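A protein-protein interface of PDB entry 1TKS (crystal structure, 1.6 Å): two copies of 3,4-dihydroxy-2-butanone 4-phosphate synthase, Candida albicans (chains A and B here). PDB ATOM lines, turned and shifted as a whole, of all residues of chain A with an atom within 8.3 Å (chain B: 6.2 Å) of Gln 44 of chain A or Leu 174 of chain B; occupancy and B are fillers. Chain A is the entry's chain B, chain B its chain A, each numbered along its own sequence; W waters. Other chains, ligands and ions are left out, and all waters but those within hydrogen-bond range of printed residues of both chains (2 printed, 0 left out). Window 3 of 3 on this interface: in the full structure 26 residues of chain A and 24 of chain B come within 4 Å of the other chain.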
ATOM      1  N   LEU A  41      -6.942 -20.525  15.554  1.00  0.00           N
ATOM      2  CA  LEU A  41      -7.598 -19.746  16.596  1.00  0.00           C
ATOM      3  C   LEU A  41      -8.892 -19.061  16.187  1.00  0.00           C
ATOM      4  O   LEU A  41      -9.552 -18.451  17.026  1.00  0.00           O
ATOM      5  CB  LEU A  41      -6.628 -18.692  17.137  1.00  0.00           C
ATOM      6  CG  LEU A  41      -5.289 -19.196  17.680  1.00  0.00           C
ATOM      7  CD1 LEU A  41      -4.430 -18.010  18.100  1.00  0.00           C
ATOM      8  CD2 LEU A  41      -5.528 -20.131  18.852  1.00  0.00           C
ATOM      9  N   ILE A  42      -9.265 -19.160  14.913  1.00  0.00           N
ATOM     10  CA  ILE A  42     -10.488 -18.504  14.459  1.00  0.00           C
ATOM     11  C   ILE A  42     -11.758 -19.189  14.950  1.00  0.00           C
ATOM     12  O   ILE A  42     -12.018 -20.354  14.658  1.00  0.00           O
ATOM     13  CB  ILE A  42     -10.521 -18.355  12.910  1.00  0.00           C
ATOM     14  CG1 ILE A  42     -11.637 -17.392  12.505  1.00  0.00           C
ATOM     15  CG2 ILE A  42     -10.718 -19.709  12.238  1.00  0.00           C
ATOM     16  CD1 ILE A  42     -11.530 -16.896  11.068  1.00  0.00           C
ATOM     17  N   THR A  43     -12.537 -18.436  15.720  1.00  0.00           N
ATOM     18  CA  THR A  43     -13.789 -18.921  16.288  1.00  0.00           C
ATOM     19  C   THR A  43     -14.960 -18.553  15.398  1.00  0.00           C
ATOM     20  O   THR A  43     -14.800 -17.838  14.411  1.00  0.00           O
ATOM     21  CB  THR A  43     -14.054 -18.280  17.662  1.00  0.00           C
ATOM     22  OG1 THR A  43     -14.109 -16.856  17.507  1.00  0.00           O
ATOM     23  CG2 THR A  43     -12.954 -18.628  18.642  1.00  0.00           C
ATOM     24  N   GLN A  44     -16.139 -19.043  15.766  1.00  0.00           N
ATOM     25  CA  GLN A  44     -17.355 -18.745  15.026  1.00  0.00           C
ATOM     26  C   GLN A  44     -17.548 -17.232  14.991  1.00  0.00           C
ATOM     27  O   GLN A  44     -17.801 -16.660  13.936  1.00  0.00           O
ATOM     28  CB  GLN A  44     -18.562 -19.401  15.706  1.00  0.00           C
ATOM     29  CG  GLN A  44     -19.861 -19.306  14.917  1.00  0.00           C
ATOM     30  CD  GLN A  44     -20.618 -18.003  15.125  1.00  0.00           C
ATOM     31  OE1 GLN A  44     -21.638 -17.763  14.480  1.00  0.00           O
ATOM     32  NE2 GLN A  44     -20.131 -17.164  16.033  1.00  0.00           N
ATOM     33  N   GLU A  45     -17.417 -16.591  16.148  1.00  0.00           N
ATOM     34  CA  GLU A  45     -17.590 -15.146  16.235  1.00  0.00           C
ATOM     35  C   GLU A  45     -16.559 -14.397  15.401  1.00  0.00           C
ATOM     36  O   GLU A  45     -16.887 -13.415  14.736  1.00  0.00           O
ATOM     37  CB  GLU A  45     -17.487 -14.663  17.686  1.00  0.00           C
ATOM     38  CG  GLU A  45     -18.546 -15.188  18.648  1.00  0.00           C
ATOM     39  CD  GLU A  45     -18.370 -16.655  18.992  1.00  0.00           C
ATOM     40  OE1 GLU A  45     -17.255 -17.191  18.817  1.00  0.00           O
ATOM     41  OE2 GLU A  45     -19.350 -17.270  19.456  1.00  0.00           O
ATOM     42  N   LYS A  46     -15.311 -14.852  15.431  1.00  0.00           N
ATOM     43  CA  LYS A  46     -14.256 -14.184  14.674  1.00  0.00           C
ATOM     44  C   LYS A  46     -14.438 -14.357  13.175  1.00  0.00           C
ATOM     45  O   LYS A  46     -14.094 -13.465  12.394  1.00  0.00           O
ATOM     46  CB  LYS A  46     -12.887 -14.697  15.116  1.00  0.00           C
ATOM     47  CG  LYS A  46     -12.486 -14.173  16.487  1.00  0.00           C
ATOM     48  CD  LYS A  46     -11.259 -14.875  17.033  1.00  0.00           C
ATOM     49  CE  LYS A  46     -10.793 -14.203  18.315  1.00  0.00           C
ATOM     50  NZ  LYS A  46      -9.610 -14.872  18.907  1.00  0.00           N
ATOM     51  N   MET A  47     -14.983 -15.503  12.775  1.00  0.00           N
ATOM     52  CA  MET A  47     -15.243 -15.756  11.360  1.00  0.00           C
ATOM     53  C   MET A  47     -16.416 -14.878  10.927  1.00  0.00           C
ATOM     54  O   MET A  47     -16.442 -14.354   9.814  1.00  0.00           O
ATOM     55  CB  MET A  47     -15.593 -17.227  11.116  1.00  0.00           C
ATOM     56  CG  MET A  47     -15.939 -17.530   9.656  1.00  0.00           C
ATOM     57  SD  MET A  47     -14.579 -17.293   8.475  1.00  0.00           S
ATOM     58  CE  MET A  47     -14.735 -15.632   7.992  1.00  0.00           C
ATOM     59  N   ALA A  48     -17.396 -14.724  11.813  1.00  0.00           N
ATOM     60  CA  ALA A  48     -18.548 -13.895  11.495  1.00  0.00           C
ATOM     61  C   ALA A  48     -18.064 -12.459  11.297  1.00  0.00           C
ATOM     62  O   ALA A  48     -18.563 -11.739  10.430  1.00  0.00           O
ATOM     63  CB  ALA A  48     -19.581 -13.956  12.613  1.00  0.00           C
ATOM     64  N   PHE A  49     -17.088 -12.051  12.106  1.00  0.00           N
ATOM     65  CA  PHE A  49     -16.522 -10.712  12.021  1.00  0.00           C
ATOM     66  C   PHE A  49     -15.788 -10.564  10.695  1.00  0.00           C
ATOM     67  O   PHE A  49     -15.980  -9.583   9.970  1.00  0.00           O
ATOM     68  CB  PHE A  49     -15.548 -10.479  13.179  1.00  0.00           C
ATOM     69  CG  PHE A  49     -14.946  -9.101  13.206  1.00  0.00           C
ATOM     70  CD1 PHE A  49     -15.604  -8.048  13.836  1.00  0.00           C
ATOM     71  CD2 PHE A  49     -13.703  -8.864  12.623  1.00  0.00           C
ATOM     72  CE1 PHE A  49     -15.031  -6.775  13.886  1.00  0.00           C
ATOM     73  CE2 PHE A  49     -13.123  -7.597  12.666  1.00  0.00           C
ATOM     74  CZ  PHE A  49     -13.789  -6.547  13.305  1.00  0.00           C
ATOM     75  N   LEU A  50     -14.954 -11.546  10.373  1.00  0.00           N
ATOM     76  CA  LEU A  50     -14.194 -11.517   9.127  1.00  0.00           C
ATOM     77  C   LEU A  50     -15.123 -11.395   7.920  1.00  0.00           C
ATOM     78  O   LEU A  50     -14.903 -10.564   7.046  1.00  0.00           O
ATOM     79  CB  LEU A  50     -13.331 -12.785   9.007  1.00  0.00           C
ATOM     80  CG  LEU A  50     -12.467 -12.892   7.743  1.00  0.00           C
ATOM     81  CD1 LEU A  50     -11.535 -11.682   7.643  1.00  0.00           C
ATOM     82  CD2 LEU A  50     -11.654 -14.176   7.782  1.00  0.00           C
ATOM     83  N   VAL A  51     -16.160 -12.228   7.875  1.00  0.00           N
ATOM     84  CA  VAL A  51     -17.113 -12.197   6.767  1.00  0.00           C
ATOM     85  C   VAL A  51     -17.869 -10.868   6.707  1.00  0.00           C
ATOM     86  O   VAL A  51     -18.024 -10.283   5.639  1.00  0.00           O
ATOM     87  CB  VAL A  51     -18.129 -13.363   6.873  1.00  0.00           C
ATOM     88  CG1 VAL A  51     -19.235 -13.205   5.839  1.00  0.00           C
ATOM     89  CG2 VAL A  51     -17.411 -14.686   6.648  1.00  0.00           C
ATOM     90  N   SER A 102     -21.749 -21.613   6.800  1.00  0.00           N
ATOM     91  CA  SER A 102     -22.011 -20.860   8.027  1.00  0.00           C
ATOM     92  C   SER A 102     -20.705 -20.417   8.682  1.00  0.00           C
ATOM     93  O   SER A 102     -19.646 -21.002   8.439  1.00  0.00           O
ATOM     94  CB  SER A 102     -22.810 -21.704   9.021  1.00  0.00           C
ATOM     95  OG  SER A 102     -22.002 -22.704   9.619  1.00  0.00           O
ATOM     96  N   ALA A 103     -20.777 -19.380   9.508  1.00  0.00           N
ATOM     97  CA  ALA A 103     -19.585 -18.897  10.192  1.00  0.00           C
ATOM     98  C   ALA A 103     -19.017 -20.037  11.037  1.00  0.00           C
ATOM     99  O   ALA A 103     -17.807 -20.252  11.075  1.00  0.00           O
ATOM    100  CB  ALA A 103     -19.937 -17.699  11.074  1.00  0.00           C
ATOM    101  N   HIS A 104     -19.903 -20.768  11.707  1.00  0.00           N
ATOM    102  CA  HIS A 104     -19.491 -21.892  12.549  1.00  0.00           C
ATOM    103  C   HIS A 104     -18.735 -22.941  11.743  1.00  0.00           C
ATOM    104  O   HIS A 104     -17.674 -23.408  12.157  1.00  0.00           O
ATOM    105  CB  HIS A 104     -20.718 -22.549  13.188  1.00  0.00           C
ATOM    106  CG  HIS A 104     -20.461 -23.930  13.711  1.00  0.00           C
ATOM    107  ND1 HIS A 104     -20.149 -24.186  15.026  1.00  0.00           N
ATOM    108  CD2 HIS A 104     -20.438 -25.128  13.077  1.00  0.00           C
ATOM    109  CE1 HIS A 104     -19.943 -25.484  15.183  1.00  0.00           C
ATOM    110  NE2 HIS A 104     -20.111 -26.075  14.018  1.00  0.00           N
ATOM    111  N   ASP A 105     -19.296 -23.313  10.596  1.00  0.00           N
ATOM    112  CA  ASP A 105     -18.693 -24.321   9.739  1.00  0.00           C
ATOM    113  C   ASP A 105     -17.375 -23.868   9.115  1.00  0.00           C
ATOM    114  O   ASP A 105     -16.389 -24.612   9.135  1.00  0.00           O
ATOM    115  CB  ASP A 105     -19.677 -24.741   8.642  1.00  0.00           C
ATOM    116  CG  ASP A 105     -20.837 -25.580   9.177  1.00  0.00           C
ATOM    117  OD1 ASP A 105     -20.948 -25.750  10.408  1.00  0.00           O
ATOM    118  OD2 ASP A 105     -21.638 -26.065   8.355  1.00  0.00           O
ATOM    119  N   ARG A 106     -17.343 -22.660   8.560  1.00  0.00           N
ATOM    120  CA  ARG A 106     -16.107 -22.174   7.957  1.00  0.00           C
ATOM    121  C   ARG A 106     -15.007 -22.029   8.998  1.00  0.00           C
ATOM    122  O   ARG A 106     -13.842 -22.289   8.705  1.00  0.00           O
ATOM    123  CB  ARG A 106     -16.333 -20.853   7.204  1.00  0.00           C
ATOM    124  CG  ARG A 106     -16.945 -21.080   5.825  1.00  0.00           C
ATOM    125  CD  ARG A 106     -16.752 -19.910   4.878  1.00  0.00           C
ATOM    126  NE  ARG A 106     -17.744 -18.853   5.053  1.00  0.00           N
ATOM    127  CZ  ARG A 106     -17.798 -17.766   4.288  1.00  0.00           C
ATOM    128  NH1 ARG A 106     -16.914 -17.606   3.310  1.00  0.00           N
ATOM    129  NH2 ARG A 106     -18.736 -16.849   4.483  1.00  0.00           N
ATOM    130  N   ALA A 107     -15.369 -21.639  10.216  1.00  0.00           N
ATOM    131  CA  ALA A 107     -14.374 -21.503  11.273  1.00  0.00           C
ATOM    132  C   ALA A 107     -13.847 -22.886  11.655  1.00  0.00           C
ATOM    133  O   ALA A 107     -12.644 -23.067  11.842  1.00  0.00           O
ATOM    134  CB  ALA A 107     -14.988 -20.817  12.490  1.00  0.00           C
ATOM    135  N   LEU A 108     -14.750 -23.859  11.764  1.00  0.00           N
ATOM    136  CA  LEU A 108     -14.367 -25.225  12.119  1.00  0.00           C
ATOM    137  C   LEU A 108     -13.448 -25.812  11.057  1.00  0.00           C
ATOM    138  O   LEU A 108     -12.445 -26.447  11.377  1.00  0.00           O
ATOM    139  CB  LEU A 108     -15.612 -26.112  12.280  1.00  0.00           C
ATOM    140  CG  LEU A 108     -15.439 -27.620  12.519  1.00  0.00           C
ATOM    141  CD1 LEU A 108     -14.533 -27.864  13.722  1.00  0.00           C
ATOM    142  CD2 LEU A 108     -16.807 -28.267  12.750  1.00  0.00           C
ATOM    143  N   ARG A 111      -9.947 -24.172  11.367  1.00  0.00           N
ATOM    144  CA  ARG A 111      -9.168 -24.676  12.494  1.00  0.00           C
ATOM    145  C   ARG A 111      -8.691 -26.095  12.187  1.00  0.00           C
ATOM    146  O   ARG A 111      -7.573 -26.480  12.544  1.00  0.00           O
ATOM    147  CB  ARG A 111     -10.005 -24.676  13.780  1.00  0.00           C
ATOM    148  CG  ARG A 111     -10.450 -23.292  14.265  1.00  0.00           C
ATOM    149  CD  ARG A 111     -10.950 -23.340  15.710  1.00  0.00           C
ATOM    150  NE  ARG A 111     -12.052 -24.286  15.887  1.00  0.00           N
ATOM    151  CZ  ARG A 111     -13.327 -24.021  15.613  1.00  0.00           C
ATOM    152  NH1 ARG A 111     -13.682 -22.826  15.151  1.00  0.00           N
ATOM    153  NH2 ARG A 111     -14.249 -24.959  15.789  1.00  0.00           N
ATOM    154  N   LEU B 167     -28.002 -14.985   2.531  1.00  0.00           N
ATOM    155  CA  LEU B 167     -28.191 -13.817   3.379  1.00  0.00           C
ATOM    156  C   LEU B 167     -27.687 -14.119   4.786  1.00  0.00           C
ATOM    157  O   LEU B 167     -27.945 -15.194   5.328  1.00  0.00           O
ATOM    158  CB  LEU B 167     -29.672 -13.419   3.435  1.00  0.00           C
ATOM    159  CG  LEU B 167     -30.160 -12.600   2.243  1.00  0.00           C
ATOM    160  CD1 LEU B 167     -31.670 -12.686   2.137  1.00  0.00           C
ATOM    161  CD2 LEU B 167     -29.699 -11.155   2.398  1.00  0.00           C
ATOM    162  N   VAL B 168     -26.958 -13.170   5.367  1.00  0.00           N
ATOM    163  CA  VAL B 168     -26.427 -13.330   6.718  1.00  0.00           C
ATOM    164  C   VAL B 168     -26.740 -12.119   7.585  1.00  0.00           C
ATOM    165  O   VAL B 168     -26.746 -10.978   7.109  1.00  0.00           O
ATOM    166  CB  VAL B 168     -24.891 -13.550   6.716  1.00  0.00           C
ATOM    167  CG1 VAL B 168     -24.547 -14.843   5.992  1.00  0.00           C
ATOM    168  CG2 VAL B 168     -24.191 -12.368   6.076  1.00  0.00           C
ATOM    169  N   ARG B 169     -26.997 -12.380   8.863  1.00  0.00           N
ATOM    170  CA  ARG B 169     -27.320 -11.337   9.838  1.00  0.00           C
ATOM    171  C   ARG B 169     -26.084 -10.516  10.202  1.00  0.00           C
ATOM    172  O   ARG B 169     -25.000 -11.065  10.392  1.00  0.00           O
ATOM    173  CB  ARG B 169     -27.888 -11.980  11.108  1.00  0.00           C
ATOM    174  CG  ARG B 169     -29.276 -12.584  10.944  1.00  0.00           C
ATOM    175  CD  ARG B 169     -29.544 -13.638  12.013  1.00  0.00           C
ATOM    176  NE  ARG B 169     -29.255 -13.147  13.355  1.00  0.00           N
ATOM    177  CZ  ARG B 169     -30.006 -12.268  14.011  1.00  0.00           C
ATOM    178  NH1 ARG B 169     -29.654 -11.872  15.228  1.00  0.00           N
ATOM    179  NH2 ARG B 169     -31.113 -11.789  13.459  1.00  0.00           N
ATOM    180  N   ASP B 170     -26.244  -9.200  10.311  1.00  0.00           N
ATOM    181  CA  ASP B 170     -25.110  -8.356  10.667  1.00  0.00           C
ATOM    182  C   ASP B 170     -24.746  -8.501  12.140  1.00  0.00           C
ATOM    183  O   ASP B 170     -23.587  -8.332  12.520  1.00  0.00           O
ATOM    184  CB  ASP B 170     -25.402  -6.877  10.385  1.00  0.00           C
ATOM    185  CG  ASP B 170     -25.629  -6.590   8.914  1.00  0.00           C
ATOM    186  OD1 ASP B 170     -24.913  -7.160   8.064  1.00  0.00           O
ATOM    187  OD2 ASP B 170     -26.520  -5.775   8.607  1.00  0.00           O
ATOM    188  N   GLU B 171     -25.729  -8.822  12.973  1.00  0.00           N
ATOM    189  CA  GLU B 171     -25.480  -8.935  14.405  1.00  0.00           C
ATOM    190  C   GLU B 171     -24.573 -10.081  14.832  1.00  0.00           C
ATOM    191  O   GLU B 171     -23.699  -9.898  15.679  1.00  0.00           O
ATOM    192  CB  GLU B 171     -26.806  -9.026  15.168  1.00  0.00           C
ATOM    193  CG  GLU B 171     -27.714  -7.820  14.951  1.00  0.00           C
ATOM    194  CD  GLU B 171     -28.764  -8.056  13.884  1.00  0.00           C
ATOM    195  OE1 GLU B 171     -28.482  -8.781  12.904  1.00  0.00           O
ATOM    196  OE2 GLU B 171     -29.877  -7.498  14.013  1.00  0.00           O
ATOM    197  N   ASP B 172     -24.755 -11.255  14.234  1.00  0.00           N
ATOM    198  CA  ASP B 172     -23.965 -12.416  14.621  1.00  0.00           C
ATOM    199  C   ASP B 172     -23.461 -13.294  13.478  1.00  0.00           C
ATOM    200  O   ASP B 172     -22.839 -14.328  13.721  1.00  0.00           O
ATOM    201  CB  ASP B 172     -24.788 -13.279  15.571  1.00  0.00           C
ATOM    202  CG  ASP B 172     -26.228 -13.412  15.120  1.00  0.00           C
ATOM    203  OD1 ASP B 172     -26.464 -13.393  13.894  1.00  0.00           O
ATOM    204  OD2 ASP B 172     -27.115 -13.544  15.985  1.00  0.00           O
ATOM    205  N   GLY B 173     -23.745 -12.902  12.242  1.00  0.00           N
ATOM    206  CA  GLY B 173     -23.283 -13.682  11.106  1.00  0.00           C
ATOM    207  C   GLY B 173     -24.063 -14.954  10.827  1.00  0.00           C
ATOM    208  O   GLY B 173     -23.656 -15.768   9.995  1.00  0.00           O
ATOM    209  N   LEU B 174     -25.180 -15.142  11.520  1.00  0.00           N
ATOM    210  CA  LEU B 174     -25.994 -16.328  11.296  1.00  0.00           C
ATOM    211  C   LEU B 174     -26.856 -16.103  10.062  1.00  0.00           C
ATOM    212  O   LEU B 174     -27.299 -14.986   9.805  1.00  0.00           O
ATOM    213  CB  LEU B 174     -26.885 -16.604  12.507  1.00  0.00           C
ATOM    214  CG  LEU B 174     -26.154 -16.746  13.843  1.00  0.00           C
ATOM    215  CD1 LEU B 174     -27.172 -17.080  14.919  1.00  0.00           C
ATOM    216  CD2 LEU B 174     -25.086 -17.827  13.761  1.00  0.00           C
ATOM    217  N   MET B 175     -27.079 -17.165   9.297  1.00  0.00           N
ATOM    218  CA  MET B 175     -27.893 -17.082   8.090  1.00  0.00           C
ATOM    219  C   MET B 175     -29.316 -16.651   8.432  1.00  0.00           C
ATOM    220  O   MET B 175     -29.864 -17.042   9.462  1.00  0.00           O
ATOM    221  CB  MET B 175     -27.901 -18.432   7.368  1.00  0.00           C
ATOM    222  CG  MET B 175     -26.766 -18.611   6.359  1.00  0.00           C
ATOM    223  SD  MET B 175     -25.094 -18.427   7.020  1.00  0.00           S
ATOM    224  CE  MET B 175     -24.152 -18.221   5.480  1.00  0.00           C
ATOM    225  N   MET B 176     -29.907 -15.836   7.566  1.00  0.00           N
ATOM    226  CA  MET B 176     -31.258 -15.345   7.791  1.00  0.00           C
ATOM    227  C   MET B 176     -32.342 -16.379   7.527  1.00  0.00           C
ATOM    228  O   MET B 176     -32.425 -16.918   6.426  1.00  0.00           O
ATOM    229  CB  MET B 176     -31.541 -14.126   6.909  1.00  0.00           C
ATOM    230  CG  MET B 176     -30.871 -12.849   7.344  1.00  0.00           C
ATOM    231  SD  MET B 176     -31.458 -11.446   6.383  1.00  0.00           S
ATOM    232  CE  MET B 176     -30.105 -10.290   6.631  1.00  0.00           C
ATOM    233  N   ASP B 180     -36.311 -13.140   9.338  1.00  0.00           N
ATOM    234  CA  ASP B 180     -35.338 -12.111   9.000  1.00  0.00           C
ATOM    235  C   ASP B 180     -35.388 -11.763   7.520  1.00  0.00           C
ATOM    236  O   ASP B 180     -35.160 -10.615   7.146  1.00  0.00           O
ATOM    237  CB  ASP B 180     -33.931 -12.560   9.394  1.00  0.00           C
ATOM    238  CG  ASP B 180     -33.644 -12.335  10.867  1.00  0.00           C
ATOM    239  OD1 ASP B 180     -32.661 -12.907  11.383  1.00  0.00           O
ATOM    240  OD2 ASP B 180     -34.399 -11.576  11.510  1.00  0.00           O
HETATM  241  O   HOH W   1     -23.441 -18.492  10.183  1.00  0.00           O
HETATM  242  O   HOH W   2     -21.416 -14.681  16.046  1.00  0.00           O
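NE of Arg 169 of chain B is in salt-bridge range of OD1 of Asp 172 of chain B, at 2.9 Å.
The backbone carbonyl oxygen (O) of Leu 174 of chain B lies within hydrogen-bond range of the backbone NH (N) of Arg 169 of chain B (2.8 Å).
The side-chain carboxylate (OD1) of Asp 172 of chain B sits close to the backbone NH (N) of Leu 174 of chain B.
Among the printed residues, pairs that only touch across the chains: Gln 44 of chain A with Asp 172 of chain B (3.7 Å), Gln 44 of chain A with Leu 174 of chain B (3.5 Å) and Ala 48 of chain A with Asp 172 of chain B (3.5 Å).
Of chain B, only Asp 172 (3.7 Å) and Leu 174 (3.5 Å) come within 4 Å of Gln 44 of chain A.
Of chain A, only Gln 44 comes within 4 Å of Leu 174 of chain B.
Of the printed residues of chain B, Ala 48 of chain A touches Asp 172.
Of the printed residues of chain A, Asp 172 of chain B touches Gln 44 (3.7 Å) and Ala 48 (3.5 Å).
Met 47 of chain A touches none of the printed residues of chain B.
The nearest printed residue of chain A that does not touch Leu 174 of chain B is Ala 103 of chain A (5.8 Å).
The nearest printed residue of chain B that does not touch Ala 48 of chain A is Gly 173 of chain B (4.01 Å).
Hydrophobic or aromatic side chains of chain A that line the printed part of chain B: Ala 48.
Hydrophobic or aromatic side chains of chain B within 4 Å of the printed part of chain A: Leu 174.
Among the printed residues, 3 pairs touch across the chains.
No position is printed for both chains.
Water W1 lies within hydrogen-bond range of the backbone carbonyl oxygen (O) of Gly 173 of chain B, the backbone NH (N) of Ala 103 of chain A and the side-chain sulfur (SD) of Met 175 of chain B.
Water W2 lies within hydrogen-bond range of the backbone carbonyl oxygen (O) of Asp 172 of chain B (2.7 Å) and the side-chain amide nitrogen (NE2) of Gln 44 of chain A (2.8 Å).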
